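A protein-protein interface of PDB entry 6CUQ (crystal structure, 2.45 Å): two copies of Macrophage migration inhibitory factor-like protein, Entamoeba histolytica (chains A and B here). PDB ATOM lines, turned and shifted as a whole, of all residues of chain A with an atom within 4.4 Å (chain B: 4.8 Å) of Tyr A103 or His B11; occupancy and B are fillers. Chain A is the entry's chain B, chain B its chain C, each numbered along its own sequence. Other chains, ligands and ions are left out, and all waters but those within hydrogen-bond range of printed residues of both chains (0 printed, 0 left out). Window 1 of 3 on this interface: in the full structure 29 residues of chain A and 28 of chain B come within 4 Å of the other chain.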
ATOM      1  N   PHE A  58      20.818   7.522   4.873  1.00  0.00           N
ATOM      2  CA  PHE A  58      20.412   7.462   6.263  1.00  0.00           C
ATOM      3  C   PHE A  58      21.202   8.510   7.021  1.00  0.00           C
ATOM      4  O   PHE A  58      22.425   8.578   6.878  1.00  0.00           O
ATOM      5  CB  PHE A  58      20.666   6.069   6.838  1.00  0.00           C
ATOM      6  CG  PHE A  58      19.588   5.594   7.726  1.00  0.00           C
ATOM      7  CD1 PHE A  58      18.578   4.793   7.237  1.00  0.00           C
ATOM      8  CD2 PHE A  58      19.568   5.958   9.058  1.00  0.00           C
ATOM      9  CE1 PHE A  58      17.572   4.348   8.068  1.00  0.00           C
ATOM     10  CE2 PHE A  58      18.558   5.516   9.896  1.00  0.00           C
ATOM     11  CZ  PHE A  58      17.559   4.716   9.398  1.00  0.00           C
ATOM     12  N   ALA A  66      18.080   0.300   3.894  1.00  0.00           N
ATOM     13  CA  ALA A  66      16.908  -0.409   3.425  1.00  0.00           C
ATOM     14  C   ALA A  66      15.683   0.175   4.099  1.00  0.00           C
ATOM     15  O   ALA A  66      15.780   0.873   5.110  1.00  0.00           O
ATOM     16  CB  ALA A  66      17.006  -1.917   3.699  1.00  0.00           C
ATOM     17  N   PHE A  67      14.532  -0.100   3.496  1.00  0.00           N
ATOM     18  CA  PHE A  67      13.224   0.129   4.089  1.00  0.00           C
ATOM     19  C   PHE A  67      12.393  -1.113   3.794  1.00  0.00           C
ATOM     20  O   PHE A  67      12.293  -1.527   2.635  1.00  0.00           O
ATOM     21  CB  PHE A  67      12.574   1.393   3.514  1.00  0.00           C
ATOM     22  CG  PHE A  67      11.266   1.749   4.153  1.00  0.00           C
ATOM     23  CD1 PHE A  67      10.065   1.425   3.545  1.00  0.00           C
ATOM     24  CD2 PHE A  67      11.242   2.422   5.362  1.00  0.00           C
ATOM     25  CE1 PHE A  67       8.860   1.752   4.142  1.00  0.00           C
ATOM     26  CE2 PHE A  67      10.046   2.765   5.963  1.00  0.00           C
ATOM     27  CZ  PHE A  67       8.855   2.431   5.352  1.00  0.00           C
ATOM     28  N   ILE A  68      11.804  -1.705   4.831  1.00  0.00           N
ATOM     29  CA  ILE A  68      11.123  -2.997   4.718  1.00  0.00           C
ATOM     30  C   ILE A  68       9.668  -2.780   5.116  1.00  0.00           C
ATOM     31  O   ILE A  68       9.371  -2.462   6.273  1.00  0.00           O
ATOM     32  CB  ILE A  68      11.783  -4.076   5.585  1.00  0.00           C
ATOM     33  CG1 ILE A  68      13.277  -4.171   5.255  1.00  0.00           C
ATOM     34  CG2 ILE A  68      11.116  -5.422   5.339  1.00  0.00           C
ATOM     35  CD1 ILE A  68      14.060  -5.123   6.142  1.00  0.00           C
ATOM     36  N   ASN A 101      20.792   1.382   9.800  1.00  0.00           N
ATOM     37  CA  ASN A 101      20.446   1.943   8.501  1.00  0.00           C
ATOM     38  C   ASN A 101      19.292   1.179   7.849  1.00  0.00           C
ATOM     39  O   ASN A 101      19.165   1.150   6.624  1.00  0.00           O
ATOM     40  CB  ASN A 101      21.669   1.962   7.585  1.00  0.00           C
ATOM     41  CG  ASN A 101      22.764   2.856   8.103  1.00  0.00           C
ATOM     42  OD1 ASN A 101      22.500   3.857   8.774  1.00  0.00           O
ATOM     43  ND2 ASN A 101      24.004   2.508   7.796  1.00  0.00           N
ATOM     44  N   ILE A 102      18.445   0.549   8.660  1.00  0.00           N
ATOM     45  CA  ILE A 102      17.271  -0.172   8.185  1.00  0.00           C
ATOM     46  C   ILE A 102      16.053   0.317   8.954  1.00  0.00           C
ATOM     47  O   ILE A 102      16.044   0.284  10.189  1.00  0.00           O
ATOM     48  CB  ILE A 102      17.425  -1.695   8.354  1.00  0.00           C
ATOM     49  CG1 ILE A 102      18.643  -2.199   7.583  1.00  0.00           C
ATOM     50  CG2 ILE A 102      16.128  -2.407   7.976  1.00  0.00           C
ATOM     51  CD1 ILE A 102      18.983  -3.634   7.835  1.00  0.00           C
ATOM     52  N   TYR A 103      15.027   0.759   8.233  1.00  0.00           N
ATOM     53  CA  TYR A 103      13.730   1.050   8.827  1.00  0.00           C
ATOM     54  C   TYR A 103      12.713   0.008   8.373  1.00  0.00           C
ATOM     55  O   TYR A 103      12.774  -0.505   7.250  1.00  0.00           O
ATOM     56  CB  TYR A 103      13.227   2.440   8.442  1.00  0.00           C
ATOM     57  CG  TYR A 103      13.753   3.571   9.283  1.00  0.00           C
ATOM     58  CD1 TYR A 103      14.297   3.343  10.533  1.00  0.00           C
ATOM     59  CD2 TYR A 103      13.698   4.877   8.818  1.00  0.00           C
ATOM     60  CE1 TYR A 103      14.773   4.389  11.297  1.00  0.00           C
ATOM     61  CE2 TYR A 103      14.174   5.918   9.562  1.00  0.00           C
ATOM     62  CZ  TYR A 103      14.712   5.681  10.804  1.00  0.00           C
ATOM     63  OH  TYR A 103      15.181   6.755  11.542  1.00  0.00           O
ATOM     64  N   LEU A 104      11.781  -0.307   9.260  1.00  0.00           N
ATOM     65  CA  LEU A 104      10.695  -1.219   8.943  1.00  0.00           C
ATOM     66  C   LEU A 104       9.362  -0.589   9.317  1.00  0.00           C
ATOM     67  O   LEU A 104       9.279   0.246  10.230  1.00  0.00           O
ATOM     68  CB  LEU A 104      10.851  -2.542   9.673  1.00  0.00           C
ATOM     69  CG  LEU A 104      12.091  -3.368   9.357  1.00  0.00           C
ATOM     70  CD1 LEU A 104      13.209  -3.067  10.362  1.00  0.00           C
ATOM     71  CD2 LEU A 104      11.723  -4.855   9.363  1.00  0.00           C
ATOM     72  N   MET B   9      11.633   9.698  13.423  1.00  0.00           N
ATOM     73  CA  MET B   9      12.059   8.706  12.441  1.00  0.00           C
ATOM     74  C   MET B   9      11.384   8.911  11.081  1.00  0.00           C
ATOM     75  O   MET B   9      10.729   8.001  10.566  1.00  0.00           O
ATOM     76  CB  MET B   9      11.805   7.291  12.943  1.00  0.00           C
ATOM     77  CG  MET B   9      12.016   7.084  14.415  1.00  0.00           C
ATOM     78  SD  MET B   9      13.556   7.829  14.958  1.00  0.00           S
ATOM     79  CE  MET B   9      14.674   6.457  14.702  1.00  0.00           C
ATOM     80  N   PRO B  10      11.545  10.075  10.459  1.00  0.00           N
ATOM     81  CA  PRO B  10      10.873  10.292   9.172  1.00  0.00           C
ATOM     82  C   PRO B  10      11.546   9.490   8.065  1.00  0.00           C
ATOM     83  O   PRO B  10      12.763   9.283   8.074  1.00  0.00           O
ATOM     84  CB  PRO B  10      11.005  11.804   8.947  1.00  0.00           C
ATOM     85  CG  PRO B  10      12.183  12.219   9.747  1.00  0.00           C
ATOM     86  CD  PRO B  10      12.344  11.242  10.881  1.00  0.00           C
ATOM     87  N   HIS B  11      10.735   9.003   7.126  1.00  0.00           N
ATOM     88  CA  HIS B  11      11.248   8.250   5.988  1.00  0.00           C
ATOM     89  C   HIS B  11      10.506   8.663   4.723  1.00  0.00           C
ATOM     90  O   HIS B  11       9.287   8.859   4.735  1.00  0.00           O
ATOM     91  CB  HIS B  11      11.113   6.726   6.189  1.00  0.00           C
ATOM     92  CG  HIS B  11      11.727   5.925   5.084  1.00  0.00           C
ATOM     93  ND1 HIS B  11      11.063   5.639   3.911  1.00  0.00           N
ATOM     94  CD2 HIS B  11      12.961   5.376   4.963  1.00  0.00           C
ATOM     95  CE1 HIS B  11      11.856   4.937   3.118  1.00  0.00           C
ATOM     96  NE2 HIS B  11      13.013   4.762   3.734  1.00  0.00           N
ATOM     97  N   ALA B  12      11.250   8.759   3.628  1.00  0.00           N
ATOM     98  CA  ALA B  12      10.698   9.112   2.330  1.00  0.00           C
ATOM     99  C   ALA B  12      11.105   8.045   1.334  1.00  0.00           C
ATOM    100  O   ALA B  12      12.299   7.841   1.091  1.00  0.00           O
ATOM    101  CB  ALA B  12      11.194  10.482   1.870  1.00  0.00           C
ATOM    102  N   LEU B  13      10.122   7.352   0.782  1.00  0.00           N
ATOM    103  CA  LEU B  13      10.337   6.424  -0.315  1.00  0.00           C
ATOM    104  C   LEU B  13       9.897   7.154  -1.572  1.00  0.00           C
ATOM    105  O   LEU B  13       8.715   7.486  -1.723  1.00  0.00           O
ATOM    106  CB  LEU B  13       9.564   5.121  -0.115  1.00  0.00           C
ATOM    107  CG  LEU B  13      10.201   3.868  -0.724  1.00  0.00           C
ATOM    108  CD1 LEU B  13       9.390   2.606  -0.359  1.00  0.00           C
ATOM    109  CD2 LEU B  13      10.390   3.997  -2.237  1.00  0.00           C
ATOM    110  N   LEU B  36      13.267  16.528   5.206  1.00  0.00           N
ATOM    111  CA  LEU B  36      12.653  15.870   6.348  1.00  0.00           C
ATOM    112  C   LEU B  36      13.116  16.518   7.637  1.00  0.00           C
ATOM    113  O   LEU B  36      12.306  16.884   8.497  1.00  0.00           O
ATOM    114  CB  LEU B  36      13.009  14.384   6.340  1.00  0.00           C
ATOM    115  CG  LEU B  36      12.311  13.585   5.245  1.00  0.00           C
ATOM    116  CD1 LEU B  36      12.729  12.105   5.275  1.00  0.00           C
ATOM    117  CD2 LEU B  36      10.803  13.735   5.387  1.00  0.00           C
ATOM    118  N   TYR B  46      18.298  10.725  11.952  1.00  0.00           N
ATOM    119  CA  TYR B  46      17.248   9.714  11.846  1.00  0.00           C
ATOM    120  C   TYR B  46      16.351   9.924  10.635  1.00  0.00           C
ATOM    121  O   TYR B  46      15.277   9.323  10.556  1.00  0.00           O
ATOM    122  CB  TYR B  46      16.430   9.632  13.136  1.00  0.00           C
ATOM    123  CG  TYR B  46      17.314   9.171  14.267  1.00  0.00           C
ATOM    124  CD1 TYR B  46      17.938   7.928  14.209  1.00  0.00           C
ATOM    125  CD2 TYR B  46      17.582   9.995  15.359  1.00  0.00           C
ATOM    126  CE1 TYR B  46      18.779   7.506  15.217  1.00  0.00           C
ATOM    127  CE2 TYR B  46      18.422   9.578  16.374  1.00  0.00           C
ATOM    128  CZ  TYR B  46      19.019   8.331  16.294  1.00  0.00           C
ATOM    129  OH  TYR B  46      19.859   7.896  17.292  1.00  0.00           O
ATOM    130  N   CYS B  47      16.729  10.812   9.725  1.00  0.00           N
ATOM    131  CA  CYS B  47      15.998  10.974   8.479  1.00  0.00           C
ATOM    132  C   CYS B  47      16.580  10.019   7.442  1.00  0.00           C
ATOM    133  O   CYS B  47      17.799   9.834   7.360  1.00  0.00           O
ATOM    134  CB  CYS B  47      16.074  12.425   7.997  1.00  0.00           C
ATOM    135  SG  CYS B  47      15.359  13.614   9.150  1.00  0.00           S
ATOM    136  N   ALA B  48      15.702   9.380   6.675  1.00  0.00           N
ATOM    137  CA  ALA B  48      16.116   8.326   5.761  1.00  0.00           C
ATOM    138  C   ALA B  48      15.347   8.455   4.454  1.00  0.00           C
ATOM    139  O   ALA B  48      14.231   8.982   4.425  1.00  0.00           O
ATOM    140  CB  ALA B  48      15.900   6.940   6.387  1.00  0.00           C
ATOM    141  N   THR B  49      15.947   7.965   3.370  1.00  0.00           N
ATOM    142  CA  THR B  49      15.324   8.104   2.061  1.00  0.00           C
ATOM    143  C   THR B  49      15.829   7.017   1.116  1.00  0.00           C
ATOM    144  O   THR B  49      17.018   6.678   1.119  1.00  0.00           O
ATOM    145  CB  THR B  49      15.587   9.496   1.464  1.00  0.00           C
ATOM    146  OG1 THR B  49      14.914  10.479   2.254  1.00  0.00           O
ATOM    147  CG2 THR B  49      15.061   9.594   0.040  1.00  0.00           C
ATOM    148  N   GLN B  50      14.904   6.472   0.325  1.00  0.00           N
ATOM    149  CA  GLN B  50      15.214   5.568  -0.776  1.00  0.00           C
ATOM    150  C   GLN B  50      14.649   6.142  -2.069  1.00  0.00           C
ATOM    151  O   GLN B  50      13.470   6.511  -2.123  1.00  0.00           O
ATOM    152  CB  GLN B  50      14.629   4.161  -0.543  1.00  0.00           C
ATOM    153  CG  GLN B  50      15.064   3.494   0.748  1.00  0.00           C
ATOM    154  CD  GLN B  50      16.561   3.321   0.809  1.00  0.00           C
ATOM    155  OE1 GLN B  50      17.218   3.196  -0.223  1.00  0.00           O
ATOM    156  NE2 GLN B  50      17.116   3.343   2.016  1.00  0.00           N
ATOM    157  N   ASP B  69       6.231   8.492  -0.873  1.00  0.00           N
ATOM    158  CA  ASP B  69       5.599   7.888   0.295  1.00  0.00           C
ATOM    159  C   ASP B  69       6.347   8.379   1.530  1.00  0.00           C
ATOM    160  O   ASP B  69       7.464   7.930   1.808  1.00  0.00           O
ATOM    161  CB  ASP B  69       5.625   6.365   0.182  1.00  0.00           C
ATOM    162  CG  ASP B  69       4.537   5.697   0.988  1.00  0.00           C
ATOM    163  OD1 ASP B  69       3.861   6.394   1.777  1.00  0.00           O
ATOM    164  OD2 ASP B  69       4.356   4.470   0.829  1.00  0.00           O
ATOM    165  N   ILE B  70       5.736   9.317   2.264  1.00  0.00           N
ATOM    166  CA  ILE B  70       6.330   9.909   3.458  1.00  0.00           C
ATOM    167  C   ILE B  70       5.730   9.253   4.691  1.00  0.00           C
ATOM    168  O   ILE B  70       4.501   9.231   4.864  1.00  0.00           O
ATOM    169  CB  ILE B  70       6.114  11.431   3.481  1.00  0.00           C
ATOM    170  CG1 ILE B  70       6.597  12.038   2.169  1.00  0.00           C
ATOM    171  CG2 ILE B  70       6.828  12.059   4.659  1.00  0.00           C
ATOM    172  CD1 ILE B  70       8.082  12.067   2.066  1.00  0.00           C
ATOM    173  N   LYS B  71       6.591   8.739   5.568  1.00  0.00           N
ATOM    174  CA  LYS B  71       6.120   8.006   6.734  1.00  0.00           C
ATOM    175  C   LYS B  71       6.975   8.332   7.951  1.00  0.00           C
ATOM    176  O   LYS B  71       8.199   8.446   7.843  1.00  0.00           O
ATOM    177  CB  LYS B  71       6.156   6.496   6.454  1.00  0.00           C
ATOM    178  CG  LYS B  71       5.171   6.034   5.381  1.00  0.00           C
ATOM    179  CD  LYS B  71       5.267   4.546   5.128  1.00  0.00           C
ATOM    180  CE  LYS B  71       3.896   3.927   4.886  1.00  0.00           C
ATOM    181  NZ  LYS B  71       3.977   2.438   4.915  1.00  0.00           N
ATOM    182  N   TRP B 114       6.849   0.378  14.101  1.00  0.00           N
ATOM    183  CA  TRP B 114       8.030   0.995  13.506  1.00  0.00           C
ATOM    184  C   TRP B 114       9.272   0.249  13.964  1.00  0.00           C
ATOM    185  O   TRP B 114       9.610   0.266  15.154  1.00  0.00           O
ATOM    186  CB  TRP B 114       8.168   2.475  13.871  1.00  0.00           C
ATOM    187  CG  TRP B 114       9.171   3.113  12.979  1.00  0.00           C
ATOM    188  CD1 TRP B 114      10.534   2.971  13.036  1.00  0.00           C
ATOM    189  CD2 TRP B 114       8.904   3.952  11.851  1.00  0.00           C
ATOM    190  NE1 TRP B 114      11.128   3.675  12.017  1.00  0.00           N
ATOM    191  CE2 TRP B 114      10.153   4.291  11.278  1.00  0.00           C
ATOM    192  CE3 TRP B 114       7.734   4.459  11.276  1.00  0.00           C
ATOM    193  CZ2 TRP B 114      10.260   5.108  10.161  1.00  0.00           C
ATOM    194  CZ3 TRP B 114       7.843   5.264  10.168  1.00  0.00           C
ATOM    195  CH2 TRP B 114       9.099   5.584   9.618  1.00  0.00           C
ATOM    196  N   GLY B 115       9.960  -0.380  13.017  1.00  0.00           N
ATOM    197  CA  GLY B 115      11.137  -1.173  13.306  1.00  0.00           C
ATOM    198  C   GLY B 115      12.421  -0.464  12.920  1.00  0.00           C
ATOM    199  O   GLY B 115      12.480   0.249  11.919  1.00  0.00           O
ATOM    200  N   TYR B 116      13.463  -0.698  13.721  1.00  0.00           N
ATOM    201  CA  TYR B 116      14.766  -0.073  13.527  1.00  0.00           C
ATOM    202  C   TYR B 116      15.847  -0.771  14.342  1.00  0.00           C
ATOM    203  O   TYR B 116      15.677  -0.974  15.549  1.00  0.00           O
ATOM    204  CB  TYR B 116      14.698   1.412  13.886  1.00  0.00           C
ATOM    205  CG  TYR B 116      16.052   2.101  14.010  1.00  0.00           C
ATOM    206  CD1 TYR B 116      16.852   2.329  12.894  1.00  0.00           C
ATOM    207  CD2 TYR B 116      16.506   2.563  15.239  1.00  0.00           C
ATOM    208  CE1 TYR B 116      18.077   2.963  13.006  1.00  0.00           C
ATOM    209  CE2 TYR B 116      17.728   3.203  15.362  1.00  0.00           C
ATOM    210  CZ  TYR B 116      18.512   3.404  14.243  1.00  0.00           C
ATOM    211  OH  TYR B 116      19.732   4.049  14.369  1.00  0.00           O
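O of Tyr B46 lies within hydrogen-bond range of OH of Tyr A103 (2.8 Å).
N of Leu A104 lies within hydrogen-bond range of O of Gly B115 (2.8 Å).
The backbone NH of Ala B48 lies within hydrogen-bond range of the backbone carbonyl oxygen of Pro B10, at 3.3 Å.
The backbone NH (N) of His B11 lies within hydrogen-bond range of the backbone carbonyl oxygen (O) of Lys B71, at 2.7 Å.
The backbone carbonyl oxygen of Ala B12 sits at hydrogen-bond distance from the backbone NH of Gln B50 (3.0 Å).
N of Tyr A103 sits at hydrogen-bond distance from O of Ala A66, 3.2 Å away.
The backbone carbonyl oxygen (O) of Ala B48 sits at hydrogen-bond distance from the backbone NH (N) of Ala B12, at 3.1 Å.
O of Asn A101 lies within hydrogen-bond range of N of Ala A66, 3.1 Å away.
Among the printed residues, pairs that only touch across the chains: Phe A58 with Cys B47, Phe A58 with Ala B48, Ala A66 with Gln B50, Phe A67 with His B11, Ile A102 with Gly B115, Ile A102 with Tyr B116, Tyr A103 with Met B9, Tyr A103 with Pro B10, Tyr A103 with His B11, Tyr A103 with Ala B48, Tyr A103 with Trp B114, Tyr A103 with Gly B115, Tyr A103 with Tyr B116 and Leu A104 with Trp B114.
Of the printed residues of chain B, Phe A67 touches His B11.
Of chain B, only Met B9, Pro B10, His B11, Tyr B46, Ala B48, Trp B114, Gly B115 and Tyr B116 come within 4 Å of Tyr A103.
Of the printed residues of chain A, Pro B10 touches Tyr A103 (3.9 Å).
His B11 touches just these residues of chain A: Phe A67 (3.4 Å) and Tyr A103 (3.96 Å).
Leu B36 touches none of the printed residues of chain A.
The nearest printed residue of chain A that does not touch His B11 is Ala A66 (5.0 Å).
The nearest printed residue of chain A that does not touch Met B9 is Phe A58 (6.3 Å).
Along chain B the printed residues that touch a printed residue of chain A span positions 9 to 116.
Hydrophobic or aromatic side chains of chain A within 4 Å of the printed part of chain B: Phe A58, Phe A67, Tyr A103 and Leu A104.
Among the printed residues, 16 pairs touch across the chains.
Among the printed residues, no Asp or Glu carboxylate lies within 4 Å of a Lys or Arg side-chain nitrogen of the other chain.
No position is printed for both chains.
Of the 16 pairs that touch across the chains among the printed residues, none has its exchanged pair printed and touching as well.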
